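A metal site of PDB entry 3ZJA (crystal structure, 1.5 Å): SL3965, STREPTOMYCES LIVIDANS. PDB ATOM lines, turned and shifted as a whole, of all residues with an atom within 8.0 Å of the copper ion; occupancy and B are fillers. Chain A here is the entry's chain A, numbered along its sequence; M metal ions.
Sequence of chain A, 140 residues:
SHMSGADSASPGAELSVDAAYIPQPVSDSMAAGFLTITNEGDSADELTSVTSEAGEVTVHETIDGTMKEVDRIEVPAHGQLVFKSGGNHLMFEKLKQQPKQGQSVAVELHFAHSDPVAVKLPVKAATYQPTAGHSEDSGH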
ATOM      1  N   MET A  30     -23.605  10.227 -26.485  1.00  0.00           N
ATOM      2  CA  MET A  30     -23.486  11.335 -25.532  1.00  0.00           C
ATOM      3  C   MET A  30     -23.709  10.849 -24.119  1.00  0.00           C
ATOM      4  O   MET A  30     -24.604  10.025 -23.875  1.00  0.00           O
ATOM      5  CB  MET A  30     -24.548  12.410 -25.802  1.00  0.00           C
ATOM      6  CG  MET A  30     -24.618  12.915 -27.213  1.00  0.00           C
ATOM      7  SD  MET A  30     -26.088  13.982 -27.341  1.00  0.00           S
ATOM      8  CE  MET A  30     -27.351  12.766 -27.701  1.00  0.00           C
ATOM      9  N   ALA A  31     -23.015  11.476 -23.177  1.00  0.00           N
ATOM     10  CA  ALA A  31     -23.160  11.102 -21.765  1.00  0.00           C
ATOM     11  C   ALA A  31     -22.712  12.245 -20.891  1.00  0.00           C
ATOM     12  O   ALA A  31     -21.919  13.052 -21.311  1.00  0.00           O
ATOM     13  CB  ALA A  31     -22.318   9.881 -21.427  1.00  0.00           C
ATOM     14  N   ALA A  32     -23.240  12.290 -19.691  1.00  0.00           N
ATOM     15  CA  ALA A  32     -22.866  13.325 -18.720  1.00  0.00           C
ATOM     16  C   ALA A  32     -22.000  12.688 -17.668  1.00  0.00           C
ATOM     17  O   ALA A  32     -22.231  11.522 -17.294  1.00  0.00           O
ATOM     18  CB  ALA A  32     -24.064  13.939 -18.098  1.00  0.00           C
ATOM     19  N   GLY A  33     -20.991  13.411 -17.227  1.00  0.00           N
ATOM     20  CA  GLY A  33     -20.075  12.933 -16.189  1.00  0.00           C
ATOM     21  C   GLY A  33     -20.083  13.886 -15.006  1.00  0.00           C
ATOM     22  O   GLY A  33     -20.154  15.119 -15.179  1.00  0.00           O
ATOM     23  N   THR A  58     -16.531  18.323 -23.026  1.00  0.00           N
ATOM     24  CA  THR A  58     -16.678  19.750 -22.788  1.00  0.00           C
ATOM     25  C   THR A  58     -17.316  19.917 -21.429  1.00  0.00           C
ATOM     26  O   THR A  58     -17.864  18.975 -20.866  1.00  0.00           O
ATOM     27  CB  THR A  58     -17.557  20.444 -23.851  1.00  0.00           C
ATOM     28  OG1 THR A  58     -18.750  19.729 -24.043  1.00  0.00           O
ATOM     29  CG2 THR A  58     -16.809  20.466 -25.181  1.00  0.00           C
ATOM     30  N   VAL A  59     -17.216  21.105 -20.856  1.00  0.00           N
ATOM     31  CA  VAL A  59     -17.845  21.466 -19.610  1.00  0.00           C
ATOM     32  C   VAL A  59     -19.145  22.189 -19.917  1.00  0.00           C
ATOM     33  O   VAL A  59     -19.140  23.154 -20.715  1.00  0.00           O
ATOM     34  CB  VAL A  59     -16.935  22.362 -18.731  1.00  0.00           C
ATOM     35  CG1 VAL A  59     -17.678  22.912 -17.537  1.00  0.00           C
ATOM     36  CG2 VAL A  59     -15.635  21.652 -18.307  1.00  0.00           C
ATOM     37  N   HIS A  60     -20.218  21.724 -19.320  1.00  0.00           N
ATOM     38  CA  HIS A  60     -21.512  22.364 -19.413  1.00  0.00           C
ATOM     39  C   HIS A  60     -22.015  22.845 -18.057  1.00  0.00           C
ATOM     40  O   HIS A  60     -21.804  22.165 -17.005  1.00  0.00           O
ATOM     41  CB  HIS A  60     -22.532  21.380 -19.903  1.00  0.00           C
ATOM     42  CG  HIS A  60     -22.446  21.106 -21.349  1.00  0.00           C
ATOM     43  ND1 HIS A  60     -23.379  20.321 -21.990  1.00  0.00           N
ATOM     44  CD2 HIS A  60     -21.595  21.521 -22.309  1.00  0.00           C
ATOM     45  CE1 HIS A  60     -23.112  20.256 -23.270  1.00  0.00           C
ATOM     46  NE2 HIS A  60     -22.025  20.987 -23.490  1.00  0.00           N
ATOM     47  N   GLU A  61     -22.737  23.973 -18.110  1.00  0.00           N
ATOM     48  CA  GLU A  61     -23.573  24.382 -16.983  1.00  0.00           C
ATOM     49  C   GLU A  61     -25.013  24.055 -17.343  1.00  0.00           C
ATOM     50  O   GLU A  61     -25.331  23.808 -18.539  1.00  0.00           O
ATOM     51  CB  GLU A  61     -23.410  25.873 -16.633  1.00  0.00           C
ATOM     52  CG  GLU A  61     -24.037  26.797 -17.654  1.00  0.00           C
ATOM     53  CD  GLU A  61     -23.900  28.271 -17.325  1.00  0.00           C
ATOM     54  OE1 GLU A  61     -23.696  28.608 -16.137  1.00  0.00           O
ATOM     55  OE2 GLU A  61     -23.991  29.084 -18.264  1.00  0.00           O
ATOM     56  N   THR A  62     -25.872  23.985 -16.344  1.00  0.00           N
ATOM     57  CA  THR A  62     -27.306  23.741 -16.559  1.00  0.00           C
ATOM     58  C   THR A  62     -28.077  24.962 -16.073  1.00  0.00           C
ATOM     59  O   THR A  62     -27.840  25.453 -14.964  1.00  0.00           O
ATOM     60  CB  THR A  62     -27.798  22.509 -15.814  1.00  0.00           C
ATOM     61  OG1 THR A  62     -27.076  21.356 -16.256  1.00  0.00           O
ATOM     62  CG2 THR A  62     -29.304  22.275 -16.110  1.00  0.00           C
ATOM     63  N   THR A  66     -31.623  23.545 -19.396  1.00  0.00           N
ATOM     64  CA  THR A  66     -30.912  23.676 -20.685  1.00  0.00           C
ATOM     65  C   THR A  66     -29.418  23.638 -20.355  1.00  0.00           C
ATOM     66  O   THR A  66     -29.005  23.997 -19.236  1.00  0.00           O
ATOM     67  CB  THR A  66     -31.194  24.966 -21.477  1.00  0.00           C
ATOM     68  OG1 THR A  66     -30.508  26.056 -20.905  1.00  0.00           O
ATOM     69  CG2 THR A  66     -32.725  25.253 -21.547  1.00  0.00           C
ATOM     70  N   MET A  67     -28.638  23.233 -21.357  1.00  0.00           N
ATOM     71  CA  MET A  67     -27.187  23.103 -21.184  1.00  0.00           C
ATOM     72  C   MET A  67     -26.449  24.195 -21.927  1.00  0.00           C
ATOM     73  O   MET A  67     -26.842  24.629 -23.006  1.00  0.00           O
ATOM     74  CB  MET A  67     -26.744  21.743 -21.657  1.00  0.00           C
ATOM     75  CG  MET A  67     -27.426  20.587 -20.904  1.00  0.00           C
ATOM     76  SD  MET A  67     -26.815  19.017 -21.634  1.00  0.00           S
ATOM     77  CE  MET A  67     -27.531  17.787 -20.510  1.00  0.00           C
ATOM     78  N   LYS A  68     -25.337  24.669 -21.370  1.00  0.00           N
ATOM     79  CA  LYS A  68     -24.553  25.707 -21.995  1.00  0.00           C
ATOM     80  C   LYS A  68     -23.084  25.395 -21.799  1.00  0.00           C
ATOM     81  O   LYS A  68     -22.667  25.212 -20.620  1.00  0.00           O
ATOM     82  CB  LYS A  68     -24.872  27.058 -21.380  1.00  0.00           C
ATOM     83  CG  LYS A  68     -24.196  28.224 -22.070  1.00  0.00           C
ATOM     84  CD  LYS A  68     -24.659  29.569 -21.533  1.00  0.00           C
ATOM     85  CE  LYS A  68     -23.699  30.648 -21.979  1.00  0.00           C
ATOM     86  NZ  LYS A  68     -23.698  30.756 -23.450  1.00  0.00           N
ATOM     87  N   GLU A  69     -22.323  25.409 -22.879  1.00  0.00           N
ATOM     88  CA  GLU A  69     -20.844  25.202 -22.805  1.00  0.00           C
ATOM     89  C   GLU A  69     -20.195  26.364 -22.053  1.00  0.00           C
ATOM     90  O   GLU A  69     -20.676  27.533 -22.070  1.00  0.00           O
ATOM     91  CB  GLU A  69     -20.236  24.978 -24.172  1.00  0.00           C
ATOM     92  CG  GLU A  69     -18.816  24.454 -24.110  1.00  0.00           C
ATOM     93  CD  GLU A  69     -18.233  24.082 -25.479  1.00  0.00           C
ATOM     94  OE1 GLU A  69     -18.971  23.519 -26.331  1.00  0.00           O
ATOM     95  OE2 GLU A  69     -17.009  24.294 -25.634  1.00  0.00           O
ATOM     96  N   GLY A  87     -26.783  20.340 -12.608  1.00  0.00           N
ATOM     97  CA  GLY A  87     -25.843  21.419 -12.444  1.00  0.00           C
ATOM     98  C   GLY A  87     -24.700  21.377 -13.434  1.00  0.00           C
ATOM     99  O   GLY A  87     -24.882  21.085 -14.643  1.00  0.00           O
ATOM    100  N   ASN A  88     -23.491  21.677 -12.951  1.00  0.00           N
ATOM    101  CA  ASN A  88     -22.342  21.588 -13.867  1.00  0.00           C
ATOM    102  C   ASN A  88     -22.074  20.111 -14.212  1.00  0.00           C
ATOM    103  O   ASN A  88     -22.295  19.228 -13.391  1.00  0.00           O
ATOM    104  CB  ASN A  88     -21.091  22.160 -13.238  1.00  0.00           C
ATOM    105  CG  ASN A  88     -21.286  23.526 -12.767  1.00  0.00           C
ATOM    106  OD1 ASN A  88     -21.873  24.392 -13.435  1.00  0.00           O
ATOM    107  ND2 ASN A  88     -20.881  23.722 -11.524  1.00  0.00           N
ATOM    108  N   HIS A  89     -21.585  19.820 -15.396  1.00  0.00           N
ATOM    109  CA  HIS A  89     -21.289  18.442 -15.732  1.00  0.00           C
ATOM    110  C   HIS A  89     -20.304  18.395 -16.857  1.00  0.00           C
ATOM    111  O   HIS A  89     -20.177  19.356 -17.663  1.00  0.00           O
ATOM    112  CB  HIS A  89     -22.555  17.626 -16.079  1.00  0.00           C
ATOM    113  CG  HIS A  89     -23.358  18.180 -17.206  1.00  0.00           C
ATOM    114  ND1 HIS A  89     -24.211  19.246 -17.035  1.00  0.00           N
ATOM    115  CD2 HIS A  89     -23.419  17.840 -18.522  1.00  0.00           C
ATOM    116  CE1 HIS A  89     -24.767  19.532 -18.202  1.00  0.00           C
ATOM    117  NE2 HIS A  89     -24.329  18.700 -19.112  1.00  0.00           N
ATOM    118  N   LEU A  90     -19.526  17.330 -16.953  1.00  0.00           N
ATOM    119  CA  LEU A  90     -18.801  17.060 -18.153  1.00  0.00           C
ATOM    120  C   LEU A  90     -19.813  16.542 -19.180  1.00  0.00           C
ATOM    121  O   LEU A  90     -20.648  15.714 -18.844  1.00  0.00           O
ATOM    122  CB  LEU A  90     -17.696  16.050 -17.902  1.00  0.00           C
ATOM    123  CG  LEU A  90     -16.716  16.420 -16.789  1.00  0.00           C
ATOM    124  CD1 LEU A  90     -15.670  15.334 -16.693  1.00  0.00           C
ATOM    125  CD2 LEU A  90     -16.078  17.789 -17.027  1.00  0.00           C
ATOM    126  N   MET A  91     -19.634  16.974 -20.428  1.00  0.00           N
ATOM    127  CA  MET A  91     -20.419  16.386 -21.490  1.00  0.00           C
ATOM    128  C   MET A  91     -19.556  15.632 -22.443  1.00  0.00           C
ATOM    129  O   MET A  91     -18.677  16.224 -23.040  1.00  0.00           O
ATOM    130  CB  MET A  91     -21.208  17.475 -22.210  1.00  0.00           C
ATOM    131  CG  MET A  91     -22.414  16.912 -22.916  1.00  0.00           C
ATOM    132  SD  MET A  91     -23.741  16.694 -21.706  1.00  0.00           S
ATOM    133  CE  MET A  91     -24.848  15.609 -22.610  1.00  0.00           C
ATOM    134  N   PHE A  92     -19.725  14.313 -22.477  1.00  0.00           N
ATOM    135  CA  PHE A  92     -19.067  13.447 -23.445  1.00  0.00           C
ATOM    136  C   PHE A  92     -19.888  13.415 -24.720  1.00  0.00           C
ATOM    137  O   PHE A  92     -21.105  13.202 -24.682  1.00  0.00           O
ATOM    138  CB  PHE A  92     -18.900  12.019 -22.920  1.00  0.00           C
ATOM    139  CG  PHE A  92     -18.026  11.933 -21.710  1.00  0.00           C
ATOM    140  CD1 PHE A  92     -18.545  12.158 -20.450  1.00  0.00           C
ATOM    141  CD2 PHE A  92     -16.686  11.647 -21.844  1.00  0.00           C
ATOM    142  CE1 PHE A  92     -17.759  12.142 -19.320  1.00  0.00           C
ATOM    143  CE2 PHE A  92     -15.898  11.549 -20.717  1.00  0.00           C
ATOM    144  CZ  PHE A  92     -16.408  11.818 -19.476  1.00  0.00           C
ATOM    145  N   GLU A  93     -19.231  13.693 -25.829  1.00  0.00           N
ATOM    146  CA  GLU A  93     -19.897  13.613 -27.104  1.00  0.00           C
ATOM    147  C   GLU A  93     -19.012  12.814 -28.089  1.00  0.00           C
ATOM    148  O   GLU A  93     -17.812  12.541 -27.888  1.00  0.00           O
ATOM    149  CB  GLU A  93     -20.290  15.008 -27.661  1.00  0.00           C
ATOM    150  CG  GLU A  93     -21.246  15.727 -26.708  1.00  0.00           C
ATOM    151  CD  GLU A  93     -21.593  17.170 -27.020  1.00  0.00           C
ATOM    152  OE1 GLU A  93     -20.787  18.110 -26.712  1.00  0.00           O
ATOM    153  OE2 GLU A  93     -22.741  17.379 -27.428  1.00  0.00           O
HETATM  154 CU    CU M   1     -24.623  18.758 -21.175  1.00  0.00          CU
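The backbone carbonyl oxygen of Gly 87 sits at hydrogen-bond distance from a ring nitrogen (ND1) of His 89, at 3.1 Å.
N of Met 91 sits at hydrogen-bond distance from O of Thr 58 (2.7 Å).
Along chain A the residues within 4 Å of the copper ion span positions 60 to 91.
The copper ion is bound by NE2 of His 89 (2.1 Å), ND1 of His 60 (2.2 Å), SD of Met 67 (2.3 Å) and SD of Met 91 (2.3 Å).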
